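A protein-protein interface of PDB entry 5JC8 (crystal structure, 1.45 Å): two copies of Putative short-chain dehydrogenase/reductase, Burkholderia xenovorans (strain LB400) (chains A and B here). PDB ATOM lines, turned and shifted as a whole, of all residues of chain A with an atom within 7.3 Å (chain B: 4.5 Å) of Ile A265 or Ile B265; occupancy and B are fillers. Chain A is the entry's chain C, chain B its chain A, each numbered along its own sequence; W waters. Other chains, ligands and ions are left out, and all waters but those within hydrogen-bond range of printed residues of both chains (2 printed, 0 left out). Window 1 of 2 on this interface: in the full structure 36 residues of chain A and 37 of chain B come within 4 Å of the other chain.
O of Ser B199 lies within hydrogen-bond range of N of Ile B265, 2.9 Å away. N of Val B201 lies within hydrogen-bond range of O of Ile B265, at 2.8 Å. ND2 of Asn A198 is in hydrogen-bond range of O of Val A260. The side-chain amide oxygen (OD1) of Asn A198 is in hydrogen-bond range of the backbone NH (N) of Thr A263, at 3.1 Å. O of Ser A199 is in hydrogen-bond range of N of Ile A265 (2.9 Å). O of Ile A265 lies within hydrogen-bond range of N of Val A201, 2.8 Å away.
Among the printed residues, pairs that only touch across the chains: Asn A247 with Phe B251 (3.6 Å), Ala A248 with Phe B251 (3.8 Å), Phe A251 with Ala B248 (3.8 Å), Val A260 with Val B266 (3.7 Å), Thr A263 with Val B266 (3.6 Å), Glu A264 with Glu B264 (3.8 Å) and Ile A265 with Ile B265 (3.8 Å).
Ile A265 touches just one residue of chain B: Ile B265 (3.8 Å). Ile B265 touches one residue of chain A. Of the printed residues of chain B, Glu A264 touches Glu B264 (3.8 Å). Printed residues of chain B within 4 Å of Thr A263: Val B266. Printed residues of chain A within 4 Å of Ala B248: Phe A251 (3.8 Å). Of the printed residues of chain A, Val B266 touches Val A260 and Thr A263. The nearest residue of chain A that does not touch Ile B265 is Phe A251 (4.4 Å).
Hydrophobic or aromatic side chains of chain B within 4 Å of the printed part of chain A: Phe B251, Ile B265 and Val B266. Hydrophobic or aromatic side chains of chain A within 4 Å of the printed part of chain B: Phe A251, Val A260 and Ile A265. Along chain A the printed residues that touch a printed residue of chain B span positions 247 to 265. Among the printed residues, 7 pairs touch across the chains. Among the printed residues, no Asp or Glu carboxylate lies within 4 Å of a Lys or Arg side-chain nitrogen of the other chain.
Ala A248 touches Phe B251, and with the chains exchanged Phe A251 touches Ala B248. Glu B264 touches its own counterpart, Glu A264. Ile B265 touches its own counterpart, Ile A265.
Water W2 lies within hydrogen-bond range of OG1 of Thr A263 (2.7 Å), O of Glu A264 (2.8 Å), N of Val B266 (2.9 Å) and O of Glu B264 (3.2 Å). Water W1 lies within hydrogen-bond range of the backbone carbonyl oxygen (O) of Glu B264 (2.8 Å), the backbone NH (N) of Val A266 (2.9 Å) and the backbone carbonyl oxygen (O) of Glu A264 (3.3 Å).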
ATOM      1  N   ASN A 155      18.857  -0.308  -2.513  1.00  0.00           N
ATOM      2  CA  ASN A 155      18.258   0.371  -1.374  1.00  0.00           C
ATOM      3  C   ASN A 155      17.020   1.108  -1.845  1.00  0.00           C
ATOM      4  O   ASN A 155      17.073   1.801  -2.862  1.00  0.00           O
ATOM      5  CB  ASN A 155      19.236   1.407  -0.825  1.00  0.00           C
ATOM      6  CG  ASN A 155      20.450   0.787  -0.220  1.00  0.00           C
ATOM      7  OD1 ASN A 155      20.363  -0.152   0.550  1.00  0.00           O
ATOM      8  ND2 ASN A 155      21.614   1.301  -0.587  1.00  0.00           N
ATOM      9  N   ASN A 198      22.936   0.272  -5.573  1.00  0.00           N
ATOM     10  CA  ASN A 198      22.241   1.433  -6.113  1.00  0.00           C
ATOM     11  C   ASN A 198      20.994   1.672  -5.278  1.00  0.00           C
ATOM     12  O   ASN A 198      20.562   0.797  -4.525  1.00  0.00           O
ATOM     13  CB  ASN A 198      21.838   1.216  -7.580  1.00  0.00           C
ATOM     14  CG  ASN A 198      23.028   1.036  -8.491  1.00  0.00           C
ATOM     15  OD1 ASN A 198      23.705   2.005  -8.844  1.00  0.00           O
ATOM     16  ND2 ASN A 198      23.273  -0.204  -8.912  1.00  0.00           N
ATOM     17  N   SER A 199      20.411   2.862  -5.407  1.00  0.00           N
ATOM     18  CA  SER A 199      19.170   3.178  -4.711  1.00  0.00           C
ATOM     19  C   SER A 199      18.057   3.507  -5.688  1.00  0.00           C
ATOM     20  O   SER A 199      18.276   4.191  -6.702  1.00  0.00           O
ATOM     21  CB  SER A 199      19.349   4.373  -3.768  1.00  0.00           C
ATOM     22  OG  SER A 199      20.377   4.107  -2.822  1.00  0.00           O
ATOM     23  N   VAL A 200      16.850   3.054  -5.367  1.00  0.00           N
ATOM     24  CA  VAL A 200      15.643   3.639  -5.942  1.00  0.00           C
ATOM     25  C   VAL A 200      15.200   4.753  -5.011  1.00  0.00           C
ATOM     26  O   VAL A 200      15.242   4.605  -3.786  1.00  0.00           O
ATOM     27  CB  VAL A 200      14.543   2.584  -6.109  1.00  0.00           C
ATOM     28  CG1 VAL A 200      13.305   3.205  -6.776  1.00  0.00           C
ATOM     29  CG2 VAL A 200      15.029   1.410  -6.932  1.00  0.00           C
ATOM     30  N   VAL A 201      14.809   5.887  -5.582  1.00  0.00           N
ATOM     31  CA  VAL A 201      14.402   7.055  -4.806  1.00  0.00           C
ATOM     32  C   VAL A 201      12.945   7.336  -5.164  1.00  0.00           C
ATOM     33  O   VAL A 201      12.661   8.176  -6.041  1.00  0.00           O
ATOM     34  CB  VAL A 201      15.326   8.257  -5.083  1.00  0.00           C
ATOM     35  CG1 VAL A 201      14.912   9.472  -4.253  1.00  0.00           C
ATOM     36  CG2 VAL A 201      16.800   7.881  -4.817  1.00  0.00           C
ATOM     37  N   PRO A 202      11.989   6.649  -4.543  1.00  0.00           N
ATOM     38  CA  PRO A 202      10.584   6.855  -4.909  1.00  0.00           C
ATOM     39  C   PRO A 202      10.058   8.160  -4.331  1.00  0.00           C
ATOM     40  O   PRO A 202      10.437   8.589  -3.234  1.00  0.00           O
ATOM     41  CB  PRO A 202       9.869   5.657  -4.267  1.00  0.00           C
ATOM     42  CG  PRO A 202      10.743   5.316  -3.079  1.00  0.00           C
ATOM     43  CD  PRO A 202      12.151   5.573  -3.548  1.00  0.00           C
ATOM     44  N   ASP A 244       5.944   0.761  -9.573  1.00  0.00           N
ATOM     45  CA  ASP A 244       6.926   1.642 -10.183  1.00  0.00           C
ATOM     46  C   ASP A 244       8.265   1.527  -9.480  1.00  0.00           C
ATOM     47  O   ASP A 244       9.310   1.420 -10.136  1.00  0.00           O
ATOM     48  CB  ASP A 244       6.367   3.054 -10.182  1.00  0.00           C
ATOM     49  CG  ASP A 244       5.097   3.130 -10.986  1.00  0.00           C
ATOM     50  OD1 ASP A 244       5.184   2.965 -12.228  1.00  0.00           O
ATOM     51  OD2 ASP A 244       4.011   3.250 -10.391  1.00  0.00           O
ATOM     52  N   ASN A 247       9.730  -1.903 -10.561  1.00  0.00           N
ATOM     53  CA  ASN A 247      10.320  -1.973 -11.895  1.00  0.00           C
ATOM     54  C   ASN A 247      11.693  -1.318 -11.943  1.00  0.00           C
ATOM     55  O   ASN A 247      12.587  -1.806 -12.637  1.00  0.00           O
ATOM     56  CB  ASN A 247       9.369  -1.381 -12.938  1.00  0.00           C
ATOM     57  CG  ASN A 247       8.389  -2.397 -13.437  1.00  0.00           C
ATOM     58  OD1 ASN A 247       8.755  -3.551 -13.669  1.00  0.00           O
ATOM     59  ND2 ASN A 247       7.132  -1.999 -13.579  1.00  0.00           N
ATOM     60  N   ALA A 248      11.884  -0.217 -11.220  1.00  0.00           N
ATOM     61  CA  ALA A 248      13.214   0.381 -11.161  1.00  0.00           C
ATOM     62  C   ALA A 248      14.176  -0.521 -10.391  1.00  0.00           C
ATOM     63  O   ALA A 248      15.338  -0.701 -10.809  1.00  0.00           O
ATOM     64  CB  ALA A 248      13.123   1.779 -10.539  1.00  0.00           C
ATOM     65  N   ALA A 249      13.709  -1.117  -9.286  1.00  0.00           N
ATOM     66  CA  ALA A 249      14.551  -2.044  -8.527  1.00  0.00           C
ATOM     67  C   ALA A 249      14.919  -3.263  -9.367  1.00  0.00           C
ATOM     68  O   ALA A 249      16.037  -3.774  -9.260  1.00  0.00           O
ATOM     69  CB  ALA A 249      13.856  -2.444  -7.227  1.00  0.00           C
ATOM     70  N   PHE A 251      15.319  -3.431 -12.711  1.00  0.00           N
ATOM     71  CA  PHE A 251      16.437  -3.065 -13.568  1.00  0.00           C
ATOM     72  C   PHE A 251      17.755  -3.074 -12.796  1.00  0.00           C
ATOM     73  O   PHE A 251      18.731  -3.716 -13.208  1.00  0.00           O
ATOM     74  CB  PHE A 251      16.195  -1.692 -14.198  1.00  0.00           C
ATOM     75  CG  PHE A 251      17.401  -1.156 -14.915  1.00  0.00           C
ATOM     76  CD1 PHE A 251      17.791  -1.672 -16.135  1.00  0.00           C
ATOM     77  CD2 PHE A 251      18.164  -0.157 -14.330  1.00  0.00           C
ATOM     78  CE1 PHE A 251      18.925  -1.184 -16.770  1.00  0.00           C
ATOM     79  CE2 PHE A 251      19.296   0.335 -14.950  1.00  0.00           C
ATOM     80  CZ  PHE A 251      19.674  -0.194 -16.173  1.00  0.00           C
ATOM     81  N   LEU A 252      17.797  -2.391 -11.658  1.00  0.00           N
ATOM     82  CA  LEU A 252      19.052  -2.246 -10.918  1.00  0.00           C
ATOM     83  C   LEU A 252      19.558  -3.576 -10.364  1.00  0.00           C
ATOM     84  O   LEU A 252      20.773  -3.741 -10.183  1.00  0.00           O
ATOM     85  CB  LEU A 252      18.859  -1.254  -9.769  1.00  0.00           C
ATOM     86  CG  LEU A 252      18.624   0.183 -10.239  1.00  0.00           C
ATOM     87  CD1 LEU A 252      18.205   0.998  -9.053  1.00  0.00           C
ATOM     88  CD2 LEU A 252      19.892   0.781 -10.876  1.00  0.00           C
ATOM     89  N   VAL A 260      26.142  -0.487 -13.777  1.00  0.00           N
ATOM     90  CA  VAL A 260      25.472   0.583 -13.047  1.00  0.00           C
ATOM     91  C   VAL A 260      25.721   0.348 -11.573  1.00  0.00           C
ATOM     92  O   VAL A 260      25.275  -0.663 -11.016  1.00  0.00           O
ATOM     93  CB  VAL A 260      23.967   0.586 -13.352  1.00  0.00           C
ATOM     94  CG1 VAL A 260      23.280   1.697 -12.578  1.00  0.00           C
ATOM     95  CG2 VAL A 260      23.734   0.738 -14.844  1.00  0.00           C
ATOM     96  N   THR A 263      24.758   4.709  -7.775  1.00  0.00           N
ATOM     97  CA  THR A 263      23.884   5.759  -8.281  1.00  0.00           C
ATOM     98  C   THR A 263      22.431   5.457  -7.914  1.00  0.00           C
ATOM     99  O   THR A 263      22.132   4.521  -7.169  1.00  0.00           O
ATOM    100  CB  THR A 263      24.156   6.014  -9.769  1.00  0.00           C
ATOM    101  OG1 THR A 263      23.576   7.276 -10.153  1.00  0.00           O
ATOM    102  CG2 THR A 263      23.596   4.903 -10.641  1.00  0.00           C
ATOM    103  N   GLU A 264      21.527   6.290  -8.426  1.00  0.00           N
ATOM    104  CA  GLU A 264      20.121   6.243  -8.069  1.00  0.00           C
ATOM    105  C   GLU A 264      19.240   6.319  -9.306  1.00  0.00           C
ATOM    106  O   GLU A 264      19.624   6.846 -10.353  1.00  0.00           O
ATOM    107  CB  GLU A 264      19.742   7.418  -7.160  1.00  0.00           C
ATOM    108  CG  GLU A 264      20.510   7.505  -5.850  1.00  0.00           C
ATOM    109  CD  GLU A 264      21.858   8.169  -5.992  1.00  0.00           C
ATOM    110  OE1 GLU A 264      21.936   9.272  -6.577  1.00  0.00           O
ATOM    111  OE2 GLU A 264      22.859   7.576  -5.539  1.00  0.00           O
ATOM    112  N   ILE A 265      18.023   5.798  -9.161  1.00  0.00           N
ATOM    113  CA  ILE A 265      16.921   6.061 -10.081  1.00  0.00           C
ATOM    114  C   ILE A 265      15.801   6.706  -9.284  1.00  0.00           C
ATOM    115  O   ILE A 265      15.207   6.071  -8.392  1.00  0.00           O
ATOM    116  CB  ILE A 265      16.406   4.792 -10.776  1.00  0.00           C
ATOM    117  CG1 ILE A 265      17.530   4.129 -11.581  1.00  0.00           C
ATOM    118  CG2 ILE A 265      15.255   5.158 -11.720  1.00  0.00           C
ATOM    119  CD1 ILE A 265      17.108   2.835 -12.280  1.00  0.00           C
ATOM    120  N   VAL A 266      15.493   7.957  -9.627  1.00  0.00           N
ATOM    121  CA  VAL A 266      14.399   8.688  -8.993  1.00  0.00           C
ATOM    122  C   VAL A 266      13.103   8.325  -9.709  1.00  0.00           C
ATOM    123  O   VAL A 266      13.017   8.393 -10.940  1.00  0.00           O
ATOM    124  CB  VAL A 266      14.674  10.196  -9.061  1.00  0.00           C
ATOM    125  CG1 VAL A 266      13.486  10.988  -8.530  1.00  0.00           C
ATOM    126  CG2 VAL A 266      15.931  10.550  -8.264  1.00  0.00           C
ATOM    127  N   VAL A 267      12.099   7.924  -8.927  1.00  0.00           N
ATOM    128  CA  VAL A 267      10.816   7.458  -9.448  1.00  0.00           C
ATOM    129  C   VAL A 267       9.737   8.336  -8.819  1.00  0.00           C
ATOM    130  O   VAL A 267       9.142   7.990  -7.792  1.00  0.00           O
ATOM    131  CB  VAL A 267      10.608   5.965  -9.111  1.00  0.00           C
ATOM    132  CG1 VAL A 267       9.291   5.447  -9.689  1.00  0.00           C
ATOM    133  CG2 VAL A 267      11.783   5.106  -9.607  1.00  0.00           C
ATOM    134  N   ASP A 268       9.488   9.497  -9.425  1.00  0.00           N
ATOM    135  CA  ASP A 268       8.694  10.510  -8.744  1.00  0.00           C
ATOM    136  C   ASP A 268       7.810  11.322  -9.681  1.00  0.00           C
ATOM    137  O   ASP A 268       7.319  12.380  -9.264  1.00  0.00           O
ATOM    138  CB  ASP A 268       9.608  11.435  -7.920  1.00  0.00           C
ATOM    139  CG  ASP A 268      10.415  12.411  -8.779  1.00  0.00           C
ATOM    140  OD1 ASP A 268      10.460  12.321 -10.025  1.00  0.00           O
ATOM    141  OD2 ASP A 268      11.034  13.292  -8.154  1.00  0.00           O
ATOM    142  N   SER B 199      17.504  11.177 -19.225  1.00  0.00           N
ATOM    143  CA  SER B 199      18.813  11.019 -19.856  1.00  0.00           C
ATOM    144  C   SER B 199      19.520   9.771 -19.350  1.00  0.00           C
ATOM    145  O   SER B 199      19.432   9.435 -18.167  1.00  0.00           O
ATOM    146  CB  SER B 199      19.734  12.222 -19.605  1.00  0.00           C
ATOM    147  OG  SER B 199      19.118  13.442 -20.024  1.00  0.00           O
ATOM    148  N   VAL B 200      20.245   9.099 -20.244  1.00  0.00           N
ATOM    149  CA  VAL B 200      21.296   8.174 -19.832  1.00  0.00           C
ATOM    150  C   VAL B 200      22.597   8.945 -19.790  1.00  0.00           C
ATOM    151  O   VAL B 200      22.868   9.768 -20.677  1.00  0.00           O
ATOM    152  CB  VAL B 200      21.377   6.959 -20.774  1.00  0.00           C
ATOM    153  CG1 VAL B 200      22.459   5.994 -20.297  1.00  0.00           C
ATOM    154  CG2 VAL B 200      20.025   6.237 -20.836  1.00  0.00           C
ATOM    155  N   VAL B 201      23.384   8.725 -18.742  1.00  0.00           N
ATOM    156  CA  VAL B 201      24.646   9.434 -18.562  1.00  0.00           C
ATOM    157  C   VAL B 201      25.764   8.394 -18.603  1.00  0.00           C
ATOM    158  O   VAL B 201      26.198   7.897 -17.552  1.00  0.00           O
ATOM    159  CB  VAL B 201      24.609  10.265 -17.270  1.00  0.00           C
ATOM    160  CG1 VAL B 201      25.908  11.037 -17.064  1.00  0.00           C
ATOM    161  CG2 VAL B 201      23.424  11.230 -17.307  1.00  0.00           C
ATOM    162  N   ALA B 248      19.964   0.707 -20.187  1.00  0.00           N
ATOM    163  CA  ALA B 248      19.390   1.799 -19.408  1.00  0.00           C
ATOM    164  C   ALA B 248      18.379   2.584 -20.235  1.00  0.00           C
ATOM    165  O   ALA B 248      17.309   2.957 -19.731  1.00  0.00           O
ATOM    166  CB  ALA B 248      20.509   2.704 -18.906  1.00  0.00           C
ATOM    167  N   PHE B 251      15.027   0.634 -20.393  1.00  0.00           N
ATOM    168  CA  PHE B 251      14.185   0.873 -19.230  1.00  0.00           C
ATOM    169  C   PHE B 251      13.472   2.223 -19.335  1.00  0.00           C
ATOM    170  O   PHE B 251      12.245   2.308 -19.181  1.00  0.00           O
ATOM    171  CB  PHE B 251      15.012   0.787 -17.947  1.00  0.00           C
ATOM    172  CG  PHE B 251      14.248   1.224 -16.729  1.00  0.00           C
ATOM    173  CD1 PHE B 251      13.263   0.420 -16.171  1.00  0.00           C
ATOM    174  CD2 PHE B 251      14.505   2.468 -16.172  1.00  0.00           C
ATOM    175  CE1 PHE B 251      12.544   0.865 -15.068  1.00  0.00           C
ATOM    176  CE2 PHE B 251      13.800   2.921 -15.055  1.00  0.00           C
ATOM    177  CZ  PHE B 251      12.800   2.110 -14.520  1.00  0.00           C
ATOM    178  N   LEU B 252      14.225   3.289 -19.618  1.00  0.00           N
ATOM    179  CA  LEU B 252      13.645   4.632 -19.598  1.00  0.00           C
ATOM    180  C   LEU B 252      12.620   4.834 -20.714  1.00  0.00           C
ATOM    181  O   LEU B 252      11.680   5.630 -20.548  1.00  0.00           O
ATOM    182  CB  LEU B 252      14.759   5.675 -19.685  1.00  0.00           C
ATOM    183  CG  LEU B 252      15.677   5.749 -18.479  1.00  0.00           C
ATOM    184  CD1 LEU B 252      16.870   6.619 -18.824  1.00  0.00           C
ATOM    185  CD2 LEU B 252      14.914   6.287 -17.279  1.00  0.00           C
ATOM    186  N   GLU B 264      17.897  11.073 -14.567  1.00  0.00           N
ATOM    187  CA  GLU B 264      18.992  10.428 -15.278  1.00  0.00           C
ATOM    188  C   GLU B 264      19.292   9.053 -14.699  1.00  0.00           C
ATOM    189  O   GLU B 264      19.026   8.764 -13.525  1.00  0.00           O
ATOM    190  CB  GLU B 264      20.279  11.255 -15.186  1.00  0.00           C
ATOM    191  CG  GLU B 264      20.134  12.665 -15.768  1.00  0.00           C
ATOM    192  CD  GLU B 264      19.548  13.659 -14.786  1.00  0.00           C
ATOM    193  OE1 GLU B 264      20.034  13.733 -13.634  1.00  0.00           O
ATOM    194  OE2 GLU B 264      18.592  14.363 -15.159  1.00  0.00           O
ATOM    195  N   ILE B 265      19.907   8.216 -15.534  1.00  0.00           N
ATOM    196  CA  ILE B 265      20.572   6.990 -15.080  1.00  0.00           C
ATOM    197  C   ILE B 265      22.029   7.078 -15.498  1.00  0.00           C
ATOM    198  O   ILE B 265      22.335   7.099 -16.704  1.00  0.00           O
ATOM    199  CB  ILE B 265      19.943   5.701 -15.634  1.00  0.00           C
ATOM    200  CG1 ILE B 265      18.481   5.593 -15.203  1.00  0.00           C
ATOM    201  CG2 ILE B 265      20.730   4.494 -15.153  1.00  0.00           C
ATOM    202  CD1 ILE B 265      17.796   4.353 -15.747  1.00  0.00           C
ATOM    203  N   VAL B 266      22.923   7.102 -14.509  1.00  0.00           N
ATOM    204  CA  VAL B 266      24.361   7.124 -14.753  1.00  0.00           C
ATOM    205  C   VAL B 266      24.842   5.690 -14.951  1.00  0.00           C
ATOM    206  O   VAL B 266      24.558   4.810 -14.124  1.00  0.00           O
ATOM    207  CB  VAL B 266      25.068   7.794 -13.565  1.00  0.00           C
ATOM    208  CG1 VAL B 266      26.585   7.721 -13.728  1.00  0.00           C
ATOM    209  CG2 VAL B 266      24.633   9.241 -13.428  1.00  0.00           C
ATOM    210  N   VAL B 267      25.572   5.459 -16.047  1.00  0.00           N
ATOM    211  CA  VAL B 267      26.021   4.134 -16.457  1.00  0.00           C
ATOM    212  C   VAL B 267      27.539   4.226 -16.575  1.00  0.00           C
ATOM    213  O   VAL B 267      28.088   4.495 -17.648  1.00  0.00           O
ATOM    214  CB  VAL B 267      25.370   3.696 -17.775  1.00  0.00           C
ATOM    215  CG1 VAL B 267      25.850   2.315 -18.196  1.00  0.00           C
ATOM    216  CG2 VAL B 267      23.835   3.691 -17.665  1.00  0.00           C
HETATM  217  O   HOH W   1      17.519   9.180 -11.216  1.00  0.00           O
HETATM  218  O   HOH W   2      21.694   7.723 -11.993  1.00  0.00           O
